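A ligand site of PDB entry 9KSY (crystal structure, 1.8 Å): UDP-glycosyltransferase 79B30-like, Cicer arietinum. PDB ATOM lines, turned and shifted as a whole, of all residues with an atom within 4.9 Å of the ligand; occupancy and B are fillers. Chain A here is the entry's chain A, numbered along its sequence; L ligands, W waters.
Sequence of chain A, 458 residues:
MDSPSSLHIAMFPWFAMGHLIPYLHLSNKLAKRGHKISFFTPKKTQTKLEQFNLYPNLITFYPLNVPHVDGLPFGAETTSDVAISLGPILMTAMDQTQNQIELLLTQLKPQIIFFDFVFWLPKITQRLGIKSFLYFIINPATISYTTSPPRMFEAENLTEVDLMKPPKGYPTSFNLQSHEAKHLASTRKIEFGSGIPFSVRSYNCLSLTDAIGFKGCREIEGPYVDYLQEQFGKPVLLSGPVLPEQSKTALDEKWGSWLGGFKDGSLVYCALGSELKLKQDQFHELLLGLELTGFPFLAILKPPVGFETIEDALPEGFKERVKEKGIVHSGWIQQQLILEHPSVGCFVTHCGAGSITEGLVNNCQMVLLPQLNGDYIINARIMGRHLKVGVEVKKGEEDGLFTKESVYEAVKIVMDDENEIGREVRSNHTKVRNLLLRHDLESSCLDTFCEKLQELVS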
ATOM      1  N   TRP A  14       9.074 -18.334  -4.967  1.00  0.00           N
ATOM      2  CA  TRP A  14       8.380 -19.617  -4.921  1.00  0.00           C
ATOM      3  C   TRP A  14       9.353 -20.758  -5.176  1.00  0.00           C
ATOM      4  O   TRP A  14      10.379 -20.604  -5.855  1.00  0.00           O
ATOM      5  CB  TRP A  14       7.220 -19.585  -5.926  1.00  0.00           C
ATOM      6  CG  TRP A  14       6.523 -20.848  -6.353  1.00  0.00           C
ATOM      7  CD1 TRP A  14       6.309 -21.264  -7.641  1.00  0.00           C
ATOM      8  CD2 TRP A  14       5.857 -21.810  -5.521  1.00  0.00           C
ATOM      9  NE1 TRP A  14       5.588 -22.426  -7.656  1.00  0.00           N
ATOM     10  CE2 TRP A  14       5.299 -22.787  -6.370  1.00  0.00           C
ATOM     11  CE3 TRP A  14       5.708 -21.956  -4.134  1.00  0.00           C
ATOM     12  CZ2 TRP A  14       4.595 -23.889  -5.881  1.00  0.00           C
ATOM     13  CZ3 TRP A  14       5.007 -23.064  -3.652  1.00  0.00           C
ATOM     14  CH2 TRP A  14       4.455 -24.011  -4.529  1.00  0.00           C
ATOM     15  N   ALA A  16      10.330 -23.165  -6.984  1.00  0.00           N
ATOM     16  CA  ALA A  16      10.232 -23.682  -8.339  1.00  0.00           C
ATOM     17  C   ALA A  16      11.461 -23.220  -9.086  1.00  0.00           C
ATOM     18  O   ALA A  16      11.927 -22.088  -8.875  1.00  0.00           O
ATOM     19  CB  ALA A  16       8.973 -23.163  -9.060  1.00  0.00           C
ATOM     20  N   HIS A  19      11.237 -19.989 -10.939  1.00  0.00           N
ATOM     21  CA  HIS A  19      11.265 -18.767 -10.155  1.00  0.00           C
ATOM     22  C   HIS A  19      12.648 -18.524  -9.551  1.00  0.00           C
ATOM     23  O   HIS A  19      13.187 -17.413  -9.615  1.00  0.00           O
ATOM     24  CB  HIS A  19      10.200 -18.815  -9.046  1.00  0.00           C
ATOM     25  CG  HIS A  19       8.795 -18.824  -9.568  1.00  0.00           C
ATOM     26  ND1 HIS A  19       7.864 -17.866  -9.226  1.00  0.00           N
ATOM     27  CD2 HIS A  19       8.176 -19.658 -10.441  1.00  0.00           C
ATOM     28  CE1 HIS A  19       6.728 -18.110  -9.848  1.00  0.00           C
ATOM     29  NE2 HIS A  19       6.896 -19.191 -10.607  1.00  0.00           N
ATOM     30  N   THR A  79       8.808 -27.559  -7.047  1.00  0.00           N
ATOM     31  CA  THR A  79       7.849 -28.164  -7.954  1.00  0.00           C
ATOM     32  C   THR A  79       8.490 -29.172  -8.894  1.00  0.00           C
ATOM     33  O   THR A  79       7.768 -29.936  -9.527  1.00  0.00           O
ATOM     34  CB  THR A  79       7.121 -27.084  -8.769  1.00  0.00           C
ATOM     35  OG1 THR A  79       8.095 -26.367  -9.536  1.00  0.00           O
ATOM     36  CG2 THR A  79       6.381 -26.115  -7.866  1.00  0.00           C
ATOM     37  N   PHE A 115       9.162 -11.128  -3.200  1.00  0.00           N
ATOM     38  CA  PHE A 115       8.507 -12.375  -2.810  1.00  0.00           C
ATOM     39  C   PHE A 115       7.485 -12.806  -3.850  1.00  0.00           C
ATOM     40  O   PHE A 115       7.059 -12.030  -4.709  1.00  0.00           O
ATOM     41  CB  PHE A 115       7.845 -12.266  -1.414  1.00  0.00           C
ATOM     42  CG  PHE A 115       6.552 -11.463  -1.417  1.00  0.00           C
ATOM     43  CD1 PHE A 115       6.595 -10.077  -1.427  1.00  0.00           C
ATOM     44  CD2 PHE A 115       5.317 -12.090  -1.424  1.00  0.00           C
ATOM     45  CE1 PHE A 115       5.421  -9.319  -1.432  1.00  0.00           C
ATOM     46  CE2 PHE A 115       4.138 -11.349  -1.431  1.00  0.00           C
ATOM     47  CZ  PHE A 115       4.180  -9.963  -1.440  1.00  0.00           C
ATOM     48  N   ASP A 116       7.111 -14.087  -3.759  1.00  0.00           N
ATOM     49  CA  ASP A 116       6.061 -14.748  -4.516  1.00  0.00           C
ATOM     50  C   ASP A 116       5.001 -15.230  -3.534  1.00  0.00           C
ATOM     51  O   ASP A 116       5.355 -15.713  -2.452  1.00  0.00           O
ATOM     52  CB  ASP A 116       6.649 -15.989  -5.214  1.00  0.00           C
ATOM     53  CG  ASP A 116       7.261 -15.682  -6.562  1.00  0.00           C
ATOM     54  OD1 ASP A 116       8.220 -16.404  -6.935  1.00  0.00           O
ATOM     55  OD2 ASP A 116       6.730 -14.812  -7.280  1.00  0.00           O
ATOM     56  N   PHE A 117       3.710 -15.108  -3.895  1.00  0.00           N
ATOM     57  CA  PHE A 117       2.633 -15.917  -3.296  1.00  0.00           C
ATOM     58  C   PHE A 117       2.255 -15.705  -1.824  1.00  0.00           C
ATOM     59  O   PHE A 117       1.100 -15.958  -1.467  1.00  0.00           O
ATOM     60  CB  PHE A 117       2.966 -17.406  -3.454  1.00  0.00           C
ATOM     61  CG  PHE A 117       2.687 -17.979  -4.824  1.00  0.00           C
ATOM     62  CD1 PHE A 117       1.467 -17.782  -5.438  1.00  0.00           C
ATOM     63  CD2 PHE A 117       3.621 -18.809  -5.430  1.00  0.00           C
ATOM     64  CE1 PHE A 117       1.196 -18.353  -6.671  1.00  0.00           C
ATOM     65  CE2 PHE A 117       3.364 -19.390  -6.661  1.00  0.00           C
ATOM     66  CZ  PHE A 117       2.145 -19.157  -7.282  1.00  0.00           C
ATOM     67  N   LEU A 134       6.243  -7.513  -4.360  1.00  0.00           N
ATOM     68  CA  LEU A 134       5.767  -8.709  -5.038  1.00  0.00           C
ATOM     69  C   LEU A 134       6.368  -8.761  -6.430  1.00  0.00           C
ATOM     70  O   LEU A 134       6.000  -7.961  -7.300  1.00  0.00           O
ATOM     71  CB  LEU A 134       4.239  -8.678  -5.071  1.00  0.00           C
ATOM     72  CG  LEU A 134       3.465  -9.759  -5.826  1.00  0.00           C
ATOM     73  CD1 LEU A 134       3.682 -11.148  -5.195  1.00  0.00           C
ATOM     74  CD2 LEU A 134       1.976  -9.377  -5.854  1.00  0.00           C
ATOM     75  N   PHE A 136       7.041 -10.683  -9.886  1.00  0.00           N
ATOM     76  CA  PHE A 136       6.588 -11.728 -10.796  1.00  0.00           C
ATOM     77  C   PHE A 136       7.603 -11.961 -11.913  1.00  0.00           C
ATOM     78  O   PHE A 136       8.042 -11.006 -12.574  1.00  0.00           O
ATOM     79  CB  PHE A 136       5.282 -11.323 -11.468  1.00  0.00           C
ATOM     80  CG  PHE A 136       4.082 -11.237 -10.560  1.00  0.00           C
ATOM     81  CD1 PHE A 136       3.321 -12.358 -10.274  1.00  0.00           C
ATOM     82  CD2 PHE A 136       3.654  -9.996 -10.072  1.00  0.00           C
ATOM     83  CE1 PHE A 136       2.191 -12.265  -9.490  1.00  0.00           C
ATOM     84  CE2 PHE A 136       2.537  -9.906  -9.294  1.00  0.00           C
ATOM     85  CZ  PHE A 136       1.786 -11.024  -9.006  1.00  0.00           C
ATOM     86  N   ILE A 138       6.412 -14.175 -14.224  1.00  0.00           N
ATOM     87  CA  ILE A 138       5.460 -14.518 -15.274  1.00  0.00           C
ATOM     88  C   ILE A 138       5.035 -13.240 -15.983  1.00  0.00           C
ATOM     89  O   ILE A 138       5.427 -12.142 -15.577  1.00  0.00           O
ATOM     90  CB  ILE A 138       4.233 -15.263 -14.721  1.00  0.00           C
ATOM     91  CG1 ILE A 138       3.533 -14.406 -13.654  1.00  0.00           C
ATOM     92  CG2 ILE A 138       4.631 -16.616 -14.160  1.00  0.00           C
ATOM     93  CD1 ILE A 138       2.048 -14.746 -13.515  1.00  0.00           C
ATOM     94  N   THR A 142      -0.652 -11.925 -18.113  1.00  0.00           N
ATOM     95  CA  THR A 142      -1.407 -13.005 -17.489  1.00  0.00           C
ATOM     96  C   THR A 142      -2.122 -12.506 -16.245  1.00  0.00           C
ATOM     97  O   THR A 142      -3.340 -12.678 -16.106  1.00  0.00           O
ATOM     98  CB  THR A 142      -0.465 -14.155 -17.148  1.00  0.00           C
ATOM     99  OG1 THR A 142       0.163 -14.597 -18.356  1.00  0.00           O
ATOM    100  CG2 THR A 142      -1.231 -15.321 -16.548  1.00  0.00           C
ATOM    101  N   ILE A 143      -1.387 -11.864 -15.331  1.00  0.00           N
ATOM    102  CA  ILE A 143      -2.006 -11.310 -14.129  1.00  0.00           C
ATOM    103  C   ILE A 143      -3.126 -10.332 -14.484  1.00  0.00           C
ATOM    104  O   ILE A 143      -4.196 -10.346 -13.863  1.00  0.00           O
ATOM    105  CB  ILE A 143      -0.926 -10.634 -13.252  1.00  0.00           C
ATOM    106  CG1 ILE A 143      -0.003 -11.704 -12.685  1.00  0.00           C
ATOM    107  CG2 ILE A 143      -1.579  -9.783 -12.141  1.00  0.00           C
ATOM    108  CD1 ILE A 143      -0.716 -12.738 -11.818  1.00  0.00           C
ATOM    109  N   THR A 146      -6.398 -12.307 -15.572  1.00  0.00           N
ATOM    110  CA  THR A 146      -7.101 -13.218 -14.675  1.00  0.00           C
ATOM    111  C   THR A 146      -7.315 -12.673 -13.271  1.00  0.00           C
ATOM    112  O   THR A 146      -8.199 -13.167 -12.569  1.00  0.00           O
ATOM    113  CB  THR A 146      -6.318 -14.529 -14.546  1.00  0.00           C
ATOM    114  OG1 THR A 146      -5.055 -14.234 -13.947  1.00  0.00           O
ATOM    115  CG2 THR A 146      -6.078 -15.176 -15.911  1.00  0.00           C
ATOM    116  N   THR A 147      -6.513 -11.681 -12.848  1.00  0.00           N
ATOM    117  CA  THR A 147      -6.431 -11.313 -11.438  1.00  0.00           C
ATOM    118  C   THR A 147      -6.591  -9.799 -11.223  1.00  0.00           C
ATOM    119  O   THR A 147      -6.348  -9.316 -10.109  1.00  0.00           O
ATOM    120  CB  THR A 147      -5.098 -11.795 -10.855  1.00  0.00           C
ATOM    121  OG1 THR A 147      -4.773 -13.078 -11.410  1.00  0.00           O
ATOM    122  CG2 THR A 147      -5.137 -11.899  -9.307  1.00  0.00           C
ATOM    123  N   PHE A 192      -5.026 -23.393  -3.428  1.00  0.00           N
ATOM    124  CA  PHE A 192      -3.581 -23.468  -3.644  1.00  0.00           C
ATOM    125  C   PHE A 192      -2.893 -23.057  -2.336  1.00  0.00           C
ATOM    126  O   PHE A 192      -2.453 -21.913  -2.180  1.00  0.00           O
ATOM    127  CB  PHE A 192      -3.146 -22.599  -4.835  1.00  0.00           C
ATOM    128  CG  PHE A 192      -1.701 -22.734  -5.202  1.00  0.00           C
ATOM    129  CD1 PHE A 192      -1.222 -23.903  -5.753  1.00  0.00           C
ATOM    130  CD2 PHE A 192      -0.817 -21.677  -5.017  1.00  0.00           C
ATOM    131  CE1 PHE A 192       0.121 -24.023  -6.107  1.00  0.00           C
ATOM    132  CE2 PHE A 192       0.511 -21.786  -5.359  1.00  0.00           C
ATOM    133  CZ  PHE A 192       0.995 -22.977  -5.902  1.00  0.00           C
ATOM    134  N   PHE A 198      -6.756 -20.246  -5.684  1.00  0.00           N
ATOM    135  CA  PHE A 198      -5.551 -19.827  -6.398  1.00  0.00           C
ATOM    136  C   PHE A 198      -5.579 -18.338  -6.756  1.00  0.00           C
ATOM    137  O   PHE A 198      -4.650 -17.602  -6.434  1.00  0.00           O
ATOM    138  CB  PHE A 198      -5.358 -20.696  -7.648  1.00  0.00           C
ATOM    139  CG  PHE A 198      -4.101 -20.375  -8.432  1.00  0.00           C
ATOM    140  CD1 PHE A 198      -2.860 -20.765  -7.972  1.00  0.00           C
ATOM    141  CD2 PHE A 198      -4.173 -19.703  -9.649  1.00  0.00           C
ATOM    142  CE1 PHE A 198      -1.676 -20.484  -8.690  1.00  0.00           C
ATOM    143  CE2 PHE A 198      -3.005 -19.429 -10.383  1.00  0.00           C
ATOM    144  CZ  PHE A 198      -1.767 -19.819  -9.909  1.00  0.00           C
ATOM    145  N   SER A 199      -6.643 -17.868  -7.409  1.00  0.00           N
ATOM    146  CA  SER A 199      -6.611 -16.459  -7.793  1.00  0.00           C
ATOM    147  C   SER A 199      -6.810 -15.543  -6.594  1.00  0.00           C
ATOM    148  O   SER A 199      -6.275 -14.423  -6.595  1.00  0.00           O
ATOM    149  CB  SER A 199      -7.656 -16.175  -8.866  1.00  0.00           C
ATOM    150  OG  SER A 199      -7.285 -16.825 -10.058  1.00  0.00           O
ATOM    151  N   SER A 202      -3.292 -14.742  -5.199  1.00  0.00           N
ATOM    152  CA  SER A 202      -2.527 -13.722  -5.907  1.00  0.00           C
ATOM    153  C   SER A 202      -3.160 -12.345  -5.776  1.00  0.00           C
ATOM    154  O   SER A 202      -2.462 -11.337  -5.721  1.00  0.00           O
ATOM    155  CB  SER A 202      -2.384 -14.093  -7.388  1.00  0.00           C
ATOM    156  OG  SER A 202      -1.538 -15.229  -7.528  1.00  0.00           O
ATOM    157  N   CYS A 205      -2.018 -10.902  -2.626  1.00  0.00           N
ATOM    158  CA  CYS A 205      -0.651 -10.404  -2.727  1.00  0.00           C
ATOM    159  C   CYS A 205      -0.611  -9.043  -3.388  1.00  0.00           C
ATOM    160  O   CYS A 205       0.027  -8.105  -2.899  1.00  0.00           O
ATOM    161  CB  CYS A 205       0.226 -11.407  -3.500  1.00  0.00           C
ATOM    162  SG  CYS A 205       0.603 -12.951  -2.648  1.00  0.00           S
ATOM    163  N   GLU A 275       8.509 -29.160 -14.709  1.00  0.00           N
ATOM    164  CA  GLU A 275       7.427 -29.497 -13.795  1.00  0.00           C
ATOM    165  C   GLU A 275       6.467 -30.534 -14.337  1.00  0.00           C
ATOM    166  O   GLU A 275       6.044 -31.413 -13.595  1.00  0.00           O
ATOM    167  CB  GLU A 275       6.640 -28.242 -13.402  1.00  0.00           C
ATOM    168  CG  GLU A 275       7.465 -27.115 -12.789  1.00  0.00           C
ATOM    169  CD  GLU A 275       6.599 -25.903 -12.480  1.00  0.00           C
ATOM    170  OE1 GLU A 275       6.597 -25.446 -11.306  1.00  0.00           O
ATOM    171  OE2 GLU A 275       5.924 -25.382 -13.408  1.00  0.00           O
ATOM    172  N   ASN A 373      -1.892 -23.950 -18.821  1.00  0.00           N
ATOM    173  CA  ASN A 373      -1.484 -23.051 -17.753  1.00  0.00           C
ATOM    174  C   ASN A 373      -1.702 -21.659 -18.314  1.00  0.00           C
ATOM    175  O   ASN A 373      -1.349 -21.404 -19.474  1.00  0.00           O
ATOM    176  CB  ASN A 373      -0.013 -23.324 -17.363  1.00  0.00           C
ATOM    177  CG  ASN A 373       0.615 -22.217 -16.539  1.00  0.00           C
ATOM    178  OD1 ASN A 373       0.825 -21.099 -17.008  1.00  0.00           O
ATOM    179  ND2 ASN A 373       1.019 -22.560 -15.319  1.00  0.00           N
ATOM    180  N   GLY A 374      -2.317 -20.768 -17.512  1.00  0.00           N
ATOM    181  CA  GLY A 374      -2.653 -19.438 -18.020  1.00  0.00           C
ATOM    182  C   GLY A 374      -1.463 -18.668 -18.587  1.00  0.00           C
ATOM    183  O   GLY A 374      -1.570 -18.036 -19.644  1.00  0.00           O
ATOM    184  N   ASP A 375      -0.318 -18.692 -17.899  1.00  0.00           N
ATOM    185  CA  ASP A 375       0.833 -17.961 -18.415  1.00  0.00           C
ATOM    186  C   ASP A 375       1.368 -18.581 -19.695  1.00  0.00           C
ATOM    187  O   ASP A 375       1.749 -17.849 -20.623  1.00  0.00           O
ATOM    188  CB  ASP A 375       1.944 -17.894 -17.367  1.00  0.00           C
ATOM    189  CG  ASP A 375       2.950 -16.774 -17.657  1.00  0.00           C
ATOM    190  OD1 ASP A 375       2.554 -15.587 -17.852  1.00  0.00           O
ATOM    191  OD2 ASP A 375       4.147 -17.102 -17.762  1.00  0.00           O
HETATM  192  C1  LIG L   1      -2.555 -18.041 -14.281  1.00  0.00           C
HETATM  193  C2  LIG L   1      -1.318 -18.642 -14.179  1.00  0.00           C
HETATM  194  C3  LIG L   1      -0.418 -18.256 -13.152  1.00  0.00           C
HETATM  195  C4  LIG L   1      -0.825 -17.248 -12.281  1.00  0.00           C
HETATM  196  C5  LIG L   1      -2.053 -16.614 -12.367  1.00  0.00           C
HETATM  197  C6  LIG L   1      -2.915 -17.039 -13.366  1.00  0.00           C
HETATM  198  C7  LIG L   1       0.894 -18.844 -12.952  1.00  0.00           C
HETATM  199  C8  LIG L   1       1.713 -18.364 -11.924  1.00  0.00           C
HETATM  200  C9  LIG L   1       1.230 -17.380 -11.065  1.00  0.00           C
HETATM  201  C10 LIG L   1       1.954 -16.732  -9.967  1.00  0.00           C
HETATM  202  C11 LIG L   1       3.350 -16.676  -9.934  1.00  0.00           C
HETATM  203  C12 LIG L   1       4.015 -15.999  -8.923  1.00  0.00           C
HETATM  204  C13 LIG L   1       3.297 -15.345  -7.945  1.00  0.00           C
HETATM  205  C14 LIG L   1       1.899 -15.364  -7.972  1.00  0.00           C
HETATM  206  C15 LIG L   1       1.240 -16.018  -9.002  1.00  0.00           C
HETATM  207  O1  LIG L   1       0.004 -16.818 -11.287  1.00  0.00           O
HETATM  208  O2  LIG L   1       1.316 -19.733 -13.742  1.00  0.00           O
HETATM  209  O3  LIG L   1       1.194 -14.720  -6.991  1.00  0.00           O
HETATM  210  O4  LIG L   1       3.909 -14.668  -6.930  1.00  0.00           O
HETATM  211  O5  LIG L   1       2.914 -18.998 -11.671  1.00  0.00           O
HETATM  212  O6  LIG L   1      -4.131 -16.445 -13.450  1.00  0.00           O
HETATM  213  O7  LIG L   1      -0.966 -19.614 -15.037  1.00  0.00           O
HETATM  214  C16 LIG L   1       2.786 -20.418 -11.532  1.00  0.00           C
HETATM  215  C17 LIG L   1       4.048 -21.033 -10.968  1.00  0.00           C
HETATM  216  C18 LIG L   1       3.879 -22.554 -10.971  1.00  0.00           C
HETATM  217  C19 LIG L   1       2.592 -22.976 -10.263  1.00  0.00           C
HETATM  218  C20 LIG L   1       1.415 -22.178 -10.778  1.00  0.00           C
HETATM  219  O8  LIG L   1       5.151 -20.702 -11.806  1.00  0.00           O
HETATM  220  O9  LIG L   1       5.009 -23.177 -10.371  1.00  0.00           O
HETATM  221  O10 LIG L   1       2.711 -22.804  -8.847  1.00  0.00           O
HETATM  222  O11 LIG L   1       1.672 -20.762 -10.731  1.00  0.00           O
HETATM  223  O   HOH W   1      -4.877 -15.727 -10.728  1.00  0.00           O
HETATM  224  O   HOH W   2       2.464 -25.713  -8.224  1.00  0.00           O
HETATM  225  O   HOH W   3       7.212 -22.487 -12.528  1.00  0.00           O
HETATM  226  O   HOH W   4      -6.258 -18.153 -12.898  1.00  0.00           O
HETATM  227  O   HOH W   5      -3.438 -21.743 -14.957  1.00  0.00           O
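N of Asp 375 sits at hydrogen-bond distance from O7 of the ligand (3.1 Å). The side-chain hydroxyl (OG) of Ser 202 sits at hydrogen-bond distance from an oxygen (O3) of the ligand, at 2.8 Å. An oxygen (O9) of the ligand lies within hydrogen-bond range of the side-chain carboxylate of Glu 275 (2.9 Å). An oxygen (O8) of the ligand is in hydrogen-bond range of a ring nitrogen (NE2) of His 19, 2.6 Å away. N of Phe 117 sits at hydrogen-bond distance from O4 of the ligand. The side-chain carboxylate (OD2) of Asp 116 lies within hydrogen-bond range of an oxygen (O4) of the ligand, 2.8 Å away. An oxygen (O6) of the ligand lies within hydrogen-bond range of the side-chain hydroxyl (OG1) of Thr 146. N of Gly 374 sits at hydrogen-bond distance from O7 of the ligand, 3.0 Å away. An oxygen (O7) of the ligand is in hydrogen-bond range of the side-chain amide oxygen (OD1) of Asn 373 (3.0 Å). NE1 of Trp 14 sits at hydrogen-bond distance from O9 of the ligand.
Merely in contact with the ligand: Leu 134, Phe 136, Ile 138, Thr 142, Thr 147, Phe 192 and Phe 198. Hydrophobic or aromatic side chains that line the ligand: Trp 14, His 19, Phe 117, Leu 134, Phe 136, Ile 138, Phe 192 and Phe 198. Within 4 Å of the ligand: Trp 14, His 19, Asp 116, Phe 117, Leu 134, Phe 136, Ile 138, Thr 142, Thr 146, Thr 147, Phe 192, Phe 198, Ser 202, Glu 275, Asn 373, Gly 374 and Asp 375.
The side-chain hydroxyl (OG1) of Thr 142 is in hydrogen-bond range of the side-chain carboxylate (OD1) of Asp 375. A ring nitrogen (ND1) of His 19 lies within hydrogen-bond range of the side-chain carboxylate (OD1) of Asp 116. The side-chain amide oxygen (OD1) of Asn 373 is in hydrogen-bond range of the backbone NH (N) of Asp 375, at 2.8 Å. O of Phe 117 sits at hydrogen-bond distance from SG of Cys 205 (3.3 Å). OE1 of Glu 275 sits at hydrogen-bond distance from OG1 of Thr 79. The side-chain carboxylate of Asp 116 lies within hydrogen-bond range of the backbone NH of Trp 14 (2.9 Å). The side-chain hydroxyl (OG1) of Thr 146 lies within hydrogen-bond range of the side-chain hydroxyl (OG1) of Thr 147, at 2.8 Å. O of Thr 142 is in hydrogen-bond range of OG1 of Thr 146.
Water W4 bridges O6 of the ligand (2.8 Å) and OG of Ser 199 (3.3 Å). Water W3 bridges an oxygen (O8) of the ligand (2.8 Å) and the side-chain carboxylate of Glu 275 (3.3 Å). Water W1 lies within hydrogen-bond range of the side-chain hydroxyl of Ser 199 (2.7 Å), the side-chain hydroxyl of Thr 147 (2.7 Å) and an oxygen (O6) of the ligand (2.9 Å). Water W5 lies within hydrogen-bond range of N of Gly 374 (3.0 Å) and O7 of the ligand (3.3 Å).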
